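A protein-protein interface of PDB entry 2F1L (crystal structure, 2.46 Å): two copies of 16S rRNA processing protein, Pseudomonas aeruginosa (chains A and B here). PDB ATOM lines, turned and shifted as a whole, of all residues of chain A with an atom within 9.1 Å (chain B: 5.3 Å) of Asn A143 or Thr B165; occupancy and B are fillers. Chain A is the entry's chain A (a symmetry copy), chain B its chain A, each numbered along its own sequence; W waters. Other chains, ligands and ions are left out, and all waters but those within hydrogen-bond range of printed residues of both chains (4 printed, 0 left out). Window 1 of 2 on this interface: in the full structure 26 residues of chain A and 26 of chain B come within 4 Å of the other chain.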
ATOM      1  N   PHE A  41     -13.092  12.433  15.556  1.00  0.00           N
ATOM      2  CA  PHE A  41     -14.269  12.035  14.775  1.00  0.00           C
ATOM      3  C   PHE A  41     -15.586  12.148  15.561  1.00  0.00           C
ATOM      4  O   PHE A  41     -16.677  11.650  15.127  1.00  0.00           O
ATOM      5  CB  PHE A  41     -14.074  10.588  14.261  1.00  0.00           C
ATOM      6  CG  PHE A  41     -12.783  10.375  13.496  1.00  0.00           C
ATOM      7  CD1 PHE A  41     -12.282  11.366  12.654  1.00  0.00           C
ATOM      8  CD2 PHE A  41     -12.102   9.169  13.576  1.00  0.00           C
ATOM      9  CE1 PHE A  41     -11.087  11.183  11.969  1.00  0.00           C
ATOM     10  CE2 PHE A  41     -10.893   8.970  12.894  1.00  0.00           C
ATOM     11  CZ  PHE A  41     -10.397   9.973  12.083  1.00  0.00           C
ATOM     12  N   ASP A  43     -18.689  14.162  17.771  1.00  0.00           N
ATOM     13  CA  ASP A  43     -19.567  15.294  17.672  1.00  0.00           C
ATOM     14  C   ASP A  43     -20.011  15.582  19.087  1.00  0.00           C
ATOM     15  O   ASP A  43     -20.552  14.720  19.720  1.00  0.00           O
ATOM     16  CB  ASP A  43     -20.783  14.922  16.839  1.00  0.00           C
ATOM     17  CG  ASP A  43     -21.692  16.078  16.613  1.00  0.00           C
ATOM     18  OD1 ASP A  43     -21.356  17.201  17.082  1.00  0.00           O
ATOM     19  OD2 ASP A  43     -22.737  15.851  15.954  1.00  0.00           O
ATOM     20  N   TRP A 115     -32.506  16.947  21.969  1.00  0.00           N
ATOM     21  CA  TRP A 115     -32.852  18.124  21.196  1.00  0.00           C
ATOM     22  C   TRP A 115     -33.270  19.303  22.073  1.00  0.00           C
ATOM     23  O   TRP A 115     -32.908  20.451  21.797  1.00  0.00           O
ATOM     24  CB  TRP A 115     -34.016  17.777  20.266  1.00  0.00           C
ATOM     25  CG  TRP A 115     -33.635  17.246  18.950  1.00  0.00           C
ATOM     26  CD1 TRP A 115     -32.416  16.722  18.552  1.00  0.00           C
ATOM     27  CD2 TRP A 115     -34.489  17.183  17.819  1.00  0.00           C
ATOM     28  NE1 TRP A 115     -32.472  16.356  17.222  1.00  0.00           N
ATOM     29  CE2 TRP A 115     -33.740  16.615  16.754  1.00  0.00           C
ATOM     30  CE3 TRP A 115     -35.828  17.555  17.596  1.00  0.00           C
ATOM     31  CZ2 TRP A 115     -34.299  16.397  15.484  1.00  0.00           C
ATOM     32  CZ3 TRP A 115     -36.380  17.348  16.331  1.00  0.00           C
ATOM     33  CH2 TRP A 115     -35.615  16.767  15.294  1.00  0.00           C
ATOM     34  N   LEU A 137     -34.372  22.108  16.331  1.00  0.00           N
ATOM     35  CA  LEU A 137     -33.572  21.203  15.522  1.00  0.00           C
ATOM     36  C   LEU A 137     -34.456  20.560  14.492  1.00  0.00           C
ATOM     37  O   LEU A 137     -35.650  20.465  14.691  1.00  0.00           O
ATOM     38  CB  LEU A 137     -32.878  20.139  16.376  1.00  0.00           C
ATOM     39  CG  LEU A 137     -31.542  20.724  16.851  1.00  0.00           C
ATOM     40  CD1 LEU A 137     -31.758  21.458  18.121  1.00  0.00           C
ATOM     41  CD2 LEU A 137     -30.484  19.687  17.044  1.00  0.00           C
ATOM     42  N   LEU A 138     -33.869  20.159  13.378  1.00  0.00           N
ATOM     43  CA  LEU A 138     -34.614  19.494  12.316  1.00  0.00           C
ATOM     44  C   LEU A 138     -34.025  18.135  12.043  1.00  0.00           C
ATOM     45  O   LEU A 138     -32.827  17.963  12.026  1.00  0.00           O
ATOM     46  CB  LEU A 138     -34.574  20.285  11.009  1.00  0.00           C
ATOM     47  CG  LEU A 138     -35.094  21.720  10.991  1.00  0.00           C
ATOM     48  CD1 LEU A 138     -34.885  22.296   9.585  1.00  0.00           C
ATOM     49  CD2 LEU A 138     -36.554  21.866  11.394  1.00  0.00           C
ATOM     50  N   GLU A 139     -34.891  17.174  11.821  1.00  0.00           N
ATOM     51  CA  GLU A 139     -34.491  15.875  11.352  1.00  0.00           C
ATOM     52  C   GLU A 139     -34.503  15.994   9.818  1.00  0.00           C
ATOM     53  O   GLU A 139     -35.440  16.539   9.244  1.00  0.00           O
ATOM     54  CB  GLU A 139     -35.489  14.880  11.925  1.00  0.00           C
ATOM     55  CG  GLU A 139     -35.169  13.395  11.816  1.00  0.00           C
ATOM     56  CD  GLU A 139     -36.388  12.559  12.193  1.00  0.00           C
ATOM     57  OE1 GLU A 139     -37.101  12.978  13.135  1.00  0.00           O
ATOM     58  OE2 GLU A 139     -36.656  11.530  11.528  1.00  0.00           O
ATOM     59  N   THR A 140     -33.459  15.497   9.169  1.00  0.00           N
ATOM     60  CA  THR A 140     -33.251  15.707   7.758  1.00  0.00           C
ATOM     61  C   THR A 140     -33.030  14.438   6.932  1.00  0.00           C
ATOM     62  O   THR A 140     -32.827  14.511   5.716  1.00  0.00           O
ATOM     63  CB  THR A 140     -31.967  16.495   7.542  1.00  0.00           C
ATOM     64  OG1 THR A 140     -30.853  15.642   7.848  1.00  0.00           O
ATOM     65  CG2 THR A 140     -31.919  17.756   8.417  1.00  0.00           C
ATOM     66  N   GLY A 141     -33.016  13.277   7.547  1.00  0.00           N
ATOM     67  CA  GLY A 141     -32.592  12.101   6.799  1.00  0.00           C
ATOM     68  C   GLY A 141     -31.069  11.965   6.675  1.00  0.00           C
ATOM     69  O   GLY A 141     -30.579  10.992   6.144  1.00  0.00           O
ATOM     70  N   ALA A 142     -30.312  12.944   7.136  1.00  0.00           N
ATOM     71  CA  ALA A 142     -28.875  12.799   7.300  1.00  0.00           C
ATOM     72  C   ALA A 142     -28.557  13.441   8.670  1.00  0.00           C
ATOM     73  O   ALA A 142     -29.248  13.202   9.629  1.00  0.00           O
ATOM     74  CB  ALA A 142     -28.148  13.505   6.132  1.00  0.00           C
ATOM     75  N   ASN A 143     -27.598  14.333   8.769  1.00  0.00           N
ATOM     76  CA  ASN A 143     -27.374  15.002  10.042  1.00  0.00           C
ATOM     77  C   ASN A 143     -28.539  15.878  10.413  1.00  0.00           C
ATOM     78  O   ASN A 143     -29.196  16.445   9.550  1.00  0.00           O
ATOM     79  CB  ASN A 143     -26.127  15.864   9.927  1.00  0.00           C
ATOM     80  CG  ASN A 143     -25.013  15.092   9.368  1.00  0.00           C
ATOM     81  OD1 ASN A 143     -24.565  14.159  10.050  1.00  0.00           O
ATOM     82  ND2 ASN A 143     -24.628  15.350   8.062  1.00  0.00           N
ATOM     83  N   ASP A 144     -28.774  16.018  11.712  1.00  0.00           N
ATOM     84  CA  ASP A 144     -29.715  17.008  12.204  1.00  0.00           C
ATOM     85  C   ASP A 144     -29.232  18.429  11.929  1.00  0.00           C
ATOM     86  O   ASP A 144     -28.032  18.696  11.890  1.00  0.00           O
ATOM     87  CB  ASP A 144     -29.904  16.820  13.694  1.00  0.00           C
ATOM     88  CG  ASP A 144     -30.568  15.513  14.032  1.00  0.00           C
ATOM     89  OD1 ASP A 144     -31.428  15.076  13.241  1.00  0.00           O
ATOM     90  OD2 ASP A 144     -30.243  14.927  15.095  1.00  0.00           O
ATOM     91  N   VAL A 145     -30.166  19.344  11.746  1.00  0.00           N
ATOM     92  CA  VAL A 145     -29.831  20.734  11.498  1.00  0.00           C
ATOM     93  C   VAL A 145     -30.323  21.556  12.645  1.00  0.00           C
ATOM     94  O   VAL A 145     -31.397  21.301  13.178  1.00  0.00           O
ATOM     95  CB  VAL A 145     -30.487  21.216  10.199  1.00  0.00           C
ATOM     96  CG1 VAL A 145     -30.442  22.721  10.100  1.00  0.00           C
ATOM     97  CG2 VAL A 145     -29.784  20.552   8.979  1.00  0.00           C
ATOM     98  N   MET A 146     -29.546  22.555  13.026  1.00  0.00           N
ATOM     99  CA  MET A 146     -29.917  23.494  14.076  1.00  0.00           C
ATOM    100  C   MET A 146     -30.403  24.764  13.449  1.00  0.00           C
ATOM    101  O   MET A 146     -29.707  25.374  12.658  1.00  0.00           O
ATOM    102  CB  MET A 146     -28.724  23.813  14.932  1.00  0.00           C
ATOM    103  CG  MET A 146     -28.189  22.620  15.639  1.00  0.00           C
ATOM    104  SD  MET A 146     -26.332  22.921  16.338  1.00  0.00           S
ATOM    105  CE  MET A 146     -25.276  23.308  14.723  1.00  0.00           C
ATOM    106  N   LEU A 162     -27.358  25.256  10.679  1.00  0.00           N
ATOM    107  CA  LEU A 162     -26.043  24.660  10.858  1.00  0.00           C
ATOM    108  C   LEU A 162     -26.209  23.174  11.040  1.00  0.00           C
ATOM    109  O   LEU A 162     -27.136  22.738  11.672  1.00  0.00           O
ATOM    110  CB  LEU A 162     -25.331  25.266  12.045  1.00  0.00           C
ATOM    111  CG  LEU A 162     -24.613  26.599  11.819  1.00  0.00           C
ATOM    112  CD1 LEU A 162     -25.536  27.669  11.334  1.00  0.00           C
ATOM    113  CD2 LEU A 162     -23.957  27.028  13.137  1.00  0.00           C
ATOM    114  N   PRO A 163     -25.310  22.391  10.459  1.00  0.00           N
ATOM    115  CA  PRO A 163     -25.339  20.939  10.636  1.00  0.00           C
ATOM    116  C   PRO A 163     -24.818  20.546  12.008  1.00  0.00           C
ATOM    117  O   PRO A 163     -23.816  21.108  12.489  1.00  0.00           O
ATOM    118  CB  PRO A 163     -24.396  20.455   9.549  1.00  0.00           C
ATOM    119  CG  PRO A 163     -23.384  21.552   9.446  1.00  0.00           C
ATOM    120  CD  PRO A 163     -24.171  22.833   9.633  1.00  0.00           C
ATOM    121  N   TYR A 164     -25.501  19.621  12.659  1.00  0.00           N
ATOM    122  CA  TYR A 164     -25.045  19.134  13.969  1.00  0.00           C
ATOM    123  C   TYR A 164     -24.047  18.019  13.697  1.00  0.00           C
ATOM    124  O   TYR A 164     -24.401  16.835  13.647  1.00  0.00           O
ATOM    125  CB  TYR A 164     -26.217  18.623  14.839  1.00  0.00           C
ATOM    126  CG  TYR A 164     -25.763  18.189  16.209  1.00  0.00           C
ATOM    127  CD1 TYR A 164     -25.508  19.107  17.207  1.00  0.00           C
ATOM    128  CD2 TYR A 164     -25.526  16.859  16.486  1.00  0.00           C
ATOM    129  CE1 TYR A 164     -25.053  18.714  18.461  1.00  0.00           C
ATOM    130  CE2 TYR A 164     -25.062  16.459  17.708  1.00  0.00           C
ATOM    131  CZ  TYR A 164     -24.831  17.390  18.704  1.00  0.00           C
ATOM    132  OH  TYR A 164     -24.372  16.951  19.939  1.00  0.00           O
ATOM    133  N   THR A 165     -22.816  18.424  13.447  1.00  0.00           N
ATOM    134  CA  THR A 165     -21.682  17.517  13.260  1.00  0.00           C
ATOM    135  C   THR A 165     -20.461  18.181  13.887  1.00  0.00           C
ATOM    136  O   THR A 165     -20.455  19.394  14.106  1.00  0.00           O
ATOM    137  CB  THR A 165     -21.332  17.345  11.792  1.00  0.00           C
ATOM    138  OG1 THR A 165     -20.885  18.606  11.256  1.00  0.00           O
ATOM    139  CG2 THR A 165     -22.527  16.870  11.012  1.00  0.00           C
ATOM    140  N   GLY A 166     -19.420  17.399  14.114  1.00  0.00           N
ATOM    141  CA  GLY A 166     -18.174  17.889  14.703  1.00  0.00           C
ATOM    142  C   GLY A 166     -17.344  18.793  13.798  1.00  0.00           C
ATOM    143  O   GLY A 166     -16.513  19.552  14.290  1.00  0.00           O
ATOM    144  N   GLN A 167     -17.538  18.713  12.481  1.00  0.00           N
ATOM    145  CA  GLN A 167     -16.896  19.657  11.618  1.00  0.00           C
ATOM    146  C   GLN A 167     -17.401  21.050  11.932  1.00  0.00           C
ATOM    147  O   GLN A 167     -16.698  22.069  11.662  1.00  0.00           O
ATOM    148  CB  GLN A 167     -17.167  19.313  10.142  1.00  0.00           C
ATOM    149  CG  GLN A 167     -16.387  20.188   9.169  1.00  0.00           C
ATOM    150  CD  GLN A 167     -16.485  19.759   7.717  1.00  0.00           C
ATOM    151  OE1 GLN A 167     -15.976  20.461   6.852  1.00  0.00           O
ATOM    152  NE2 GLN A 167     -17.107  18.616   7.439  1.00  0.00           N
ATOM    153  N   CYS A 168     -18.625  21.092  12.478  1.00  0.00           N
ATOM    154  CA  CYS A 168     -19.307  22.339  12.801  1.00  0.00           C
ATOM    155  C   CYS A 168     -19.351  22.670  14.306  1.00  0.00           C
ATOM    156  O   CYS A 168     -18.959  23.776  14.747  1.00  0.00           O
ATOM    157  CB  CYS A 168     -20.729  22.316  12.272  1.00  0.00           C
ATOM    158  SG  CYS A 168     -21.596  23.869  12.640  1.00  0.00           S
ATOM    159  N   PHE B  41     -29.692  19.833   2.802  1.00  0.00           N
ATOM    160  CA  PHE B  41     -29.361  19.083   4.019  1.00  0.00           C
ATOM    161  C   PHE B  41     -29.056  17.599   3.754  1.00  0.00           C
ATOM    162  O   PHE B  41     -28.960  16.749   4.701  1.00  0.00           O
ATOM    163  CB  PHE B  41     -30.524  19.219   5.031  1.00  0.00           C
ATOM    164  CG  PHE B  41     -30.915  20.652   5.333  1.00  0.00           C
ATOM    165  CD1 PHE B  41     -29.947  21.651   5.418  1.00  0.00           C
ATOM    166  CD2 PHE B  41     -32.237  20.989   5.583  1.00  0.00           C
ATOM    167  CE1 PHE B  41     -30.303  22.970   5.670  1.00  0.00           C
ATOM    168  CE2 PHE B  41     -32.613  22.316   5.836  1.00  0.00           C
ATOM    169  CZ  PHE B  41     -31.644  23.299   5.893  1.00  0.00           C
ATOM    170  N   ASP B  43     -26.929  14.263   2.048  1.00  0.00           N
ATOM    171  CA  ASP B  43     -25.595  13.749   1.911  1.00  0.00           C
ATOM    172  C   ASP B  43     -25.655  12.777   0.756  1.00  0.00           C
ATOM    173  O   ASP B  43     -26.427  11.861   0.800  1.00  0.00           O
ATOM    174  CB  ASP B  43     -25.212  12.993   3.173  1.00  0.00           C
ATOM    175  CG  ASP B  43     -23.804  12.513   3.141  1.00  0.00           C
ATOM    176  OD1 ASP B  43     -23.097  12.802   2.136  1.00  0.00           O
ATOM    177  OD2 ASP B  43     -23.412  11.855   4.138  1.00  0.00           O
ATOM    178  N   ASN B 143     -20.624  10.563  12.391  1.00  0.00           N
ATOM    179  CA  ASN B 143     -20.542  10.309  10.961  1.00  0.00           C
ATOM    180  C   ASN B 143     -19.486   9.285  10.646  1.00  0.00           C
ATOM    181  O   ASN B 143     -18.471   9.204  11.324  1.00  0.00           O
ATOM    182  CB  ASN B 143     -20.194  11.609  10.253  1.00  0.00           C
ATOM    183  CG  ASN B 143     -21.078  12.692  10.694  1.00  0.00           C
ATOM    184  OD1 ASN B 143     -22.278  12.605  10.400  1.00  0.00           O
ATOM    185  ND2 ASN B 143     -20.556  13.663  11.532  1.00  0.00           N
ATOM    186  N   PRO B 163     -14.957  13.284   6.602  1.00  0.00           N
ATOM    187  CA  PRO B 163     -16.275  12.912   7.120  1.00  0.00           C
ATOM    188  C   PRO B 163     -17.258  12.677   5.986  1.00  0.00           C
ATOM    189  O   PRO B 163     -17.284  13.439   5.001  1.00  0.00           O
ATOM    190  CB  PRO B 163     -16.671  14.136   7.924  1.00  0.00           C
ATOM    191  CG  PRO B 163     -16.038  15.268   7.180  1.00  0.00           C
ATOM    192  CD  PRO B 163     -14.701  14.732   6.709  1.00  0.00           C
ATOM    193  N   TYR B 164     -18.042  11.617   6.090  1.00  0.00           N
ATOM    194  CA  TYR B 164     -19.064  11.336   5.071  1.00  0.00           C
ATOM    195  C   TYR B 164     -20.302  12.126   5.467  1.00  0.00           C
ATOM    196  O   TYR B 164     -21.195  11.621   6.159  1.00  0.00           O
ATOM    197  CB  TYR B 164     -19.383   9.826   4.970  1.00  0.00           C
ATOM    198  CG  TYR B 164     -20.379   9.527   3.879  1.00  0.00           C
ATOM    199  CD1 TYR B 164     -19.999   9.469   2.554  1.00  0.00           C
ATOM    200  CD2 TYR B 164     -21.717   9.364   4.169  1.00  0.00           C
ATOM    201  CE1 TYR B 164     -20.920   9.229   1.540  1.00  0.00           C
ATOM    202  CE2 TYR B 164     -22.637   9.146   3.183  1.00  0.00           C
ATOM    203  CZ  TYR B 164     -22.237   9.071   1.862  1.00  0.00           C
ATOM    204  OH  TYR B 164     -23.193   8.835   0.883  1.00  0.00           O
ATOM    205  N   THR B 165     -20.301  13.388   5.084  1.00  0.00           N
ATOM    206  CA  THR B 165     -21.435  14.296   5.269  1.00  0.00           C
ATOM    207  C   THR B 165     -21.497  15.203   4.045  1.00  0.00           C
ATOM    208  O   THR B 165     -20.513  15.332   3.316  1.00  0.00           O
ATOM    209  CB  THR B 165     -21.222  15.231   6.448  1.00  0.00           C
ATOM    210  OG1 THR B 165     -20.101  16.095   6.176  1.00  0.00           O
ATOM    211  CG2 THR B 165     -20.953  14.450   7.704  1.00  0.00           C
ATOM    212  N   GLY B 166     -22.625  15.866   3.863  1.00  0.00           N
ATOM    213  CA  GLY B 166     -22.836  16.780   2.740  1.00  0.00           C
ATOM    214  C   GLY B 166     -22.040  18.079   2.807  1.00  0.00           C
ATOM    215  O   GLY B 166     -21.835  18.723   1.782  1.00  0.00           O
ATOM    216  N   GLN B 167     -21.603  18.487   4.000  1.00  0.00           N
ATOM    217  CA  GLN B 167     -20.719  19.611   4.076  1.00  0.00           C
ATOM    218  C   GLN B 167     -19.428  19.284   3.357  1.00  0.00           C
ATOM    219  O   GLN B 167     -18.697  20.208   2.889  1.00  0.00           O
ATOM    220  CB  GLN B 167     -20.433  19.976   5.545  1.00  0.00           C
ATOM    221  CG  GLN B 167     -19.622  21.256   5.699  1.00  0.00           C
ATOM    222  CD  GLN B 167     -19.480  21.746   7.127  1.00  0.00           C
ATOM    223  OE1 GLN B 167     -18.760  22.708   7.359  1.00  0.00           O
ATOM    224  NE2 GLN B 167     -20.165  21.117   8.079  1.00  0.00           N
ATOM    225  N   CYS B 168     -19.138  17.976   3.293  1.00  0.00           N
ATOM    226  CA  CYS B 168     -17.913  17.465   2.689  1.00  0.00           C
ATOM    227  C   CYS B 168     -18.109  16.810   1.309  1.00  0.00           C
ATOM    228  O   CYS B 168     -17.428  17.157   0.314  1.00  0.00           O
ATOM    229  CB  CYS B 168     -17.252  16.457   3.611  1.00  0.00           C
ATOM    230  SG  CYS B 168     -15.710  15.818   2.895  1.00  0.00           S
ATOM    231  N   VAL B 169     -19.016  15.841   1.250  1.00  0.00           N
ATOM    232  CA  VAL B 169     -19.235  15.085   0.005  1.00  0.00           C
ATOM    233  C   VAL B 169     -20.231  15.839  -0.832  1.00  0.00           C
ATOM    234  O   VAL B 169     -21.391  15.946  -0.458  1.00  0.00           O
ATOM    235  CB  VAL B 169     -19.769  13.656   0.270  1.00  0.00           C
ATOM    236  CG1 VAL B 169     -20.040  12.924  -1.076  1.00  0.00           C
ATOM    237  CG2 VAL B 169     -18.775  12.889   1.082  1.00  0.00           C
HETATM  238  O   HOH W   1     -17.564  11.466  12.628  1.00  0.00           O
HETATM  239  O   HOH W   2     -15.728  20.464   4.021  1.00  0.00           O
HETATM  240  O   HOH W   3     -27.976  17.066   7.149  1.00  0.00           O
HETATM  241  O   HOH W   4     -17.905  24.200   9.621  1.00  0.00           O
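Asn A143 touches its own counterpart, Asn B143. Asn A143 touches Thr B165, and with the chains exchanged Thr A165 touches Asn B143. Pro A163 touches Gln B167, and with the chains exchanged Gln A167 touches Pro B163. Gln A167 touches its own counterpart, Gln B167. Positions printed for both chains: 41, 43, 143, 163, 164, 165, 166, 167 and 168. Of the 9 pairs that touch across the chains among the printed residues, 6 have their exchanged pair printed and touching as well.
Water W3 lies within hydrogen-bond range of the backbone carbonyl oxygen (O) of Phe B41 (2.7 Å), the backbone carbonyl oxygen (O) of Asn A143 (2.8 Å) and the side-chain hydroxyl (OG1) of Thr A140 (3.3 Å). Water W1 lies within hydrogen-bond range of the backbone carbonyl oxygen (O) of Phe A41 (2.7 Å) and the backbone carbonyl oxygen (O) of Asn B143 (2.8 Å). Water W4 bridges OE1 of Gln B167 (2.8 Å) and O of Gln A167 (3.2 Å). Water W2 lies within hydrogen-bond range of OE1 of Gln A167 (2.8 Å) and O of Gln B167 (3.2 Å).
Of the 10 printed residues of chain B, 5 touch a printed residue of chain A. Hydrophobic or aromatic side chains of chain B within 4 Å of the printed part of chain A: Phe B41 and Pro B163. Along chain A the printed residues that touch a printed residue of chain B span positions 140 to 167. Among the printed residues, 9 pairs touch across the chains. Among the printed residues, no Asp or Glu carboxylate lies within 4 Å of a Lys or Arg side-chain nitrogen of the other chain.
Thr A140 touches Phe B41. Ala A142 touches Phe B41 (CB to O, 3.6 Å). CB of Thr B165 touches ND2 of Asn A143 (3.8 Å). Val A145 touches Phe B41 (CG2 to CD1, 3.7 Å). Pro A163 touches Gln B167 (CG to NE2, 3.5 Å). Thr A165 touches Asn B143. Gln A167 touches Pro B163 (NE2 to CG, 3.5 Å). OE1 of Gln A167 touches OE1 of Gln B167, 3.6 Å away.
The backbone carbonyl oxygen (O) of Pro B163 sits close to the side-chain sulfur (SG) of Cys B168. The backbone NH (N) of Leu A138 lies within hydrogen-bond range of the backbone carbonyl oxygen (O) of Val A145, at 2.7 Å. The side-chain hydroxyl of Thr A140 lies within hydrogen-bond range of the backbone NH of Ala A142 (2.8 Å). The side-chain hydroxyl of Thr A140 is in hydrogen-bond range of the backbone carbonyl oxygen of Asn A143, 2.5 Å away. SG of Cys A168 sits close to O of Pro A163, 3.5 Å away.
Printed residues of chain B within 4 Å of Asn A143: Asn B143 and Thr B165. Gly B166 touches none of the printed residues of chain A. No residue of chain A comes within 4 Å of Cys B168. No residue of chain A comes within 4 Å of Val B169. Of the printed residues of chain B, Ala A142 touches Phe B41. Printed residues of chain A within 4 Å of Phe B41: Thr A140 (3.8 Å), Ala A142 (3.6 Å) and Val A145 (3.7 Å). The nearest printed residue of chain B that does not touch Asn A143 is Gly B166 (4.7 Å).
The side-chain amide oxygen (OD1) of Asn B143 sits close to the side-chain amide oxygen (OD1) of Asn A143, 2.8 Å away.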
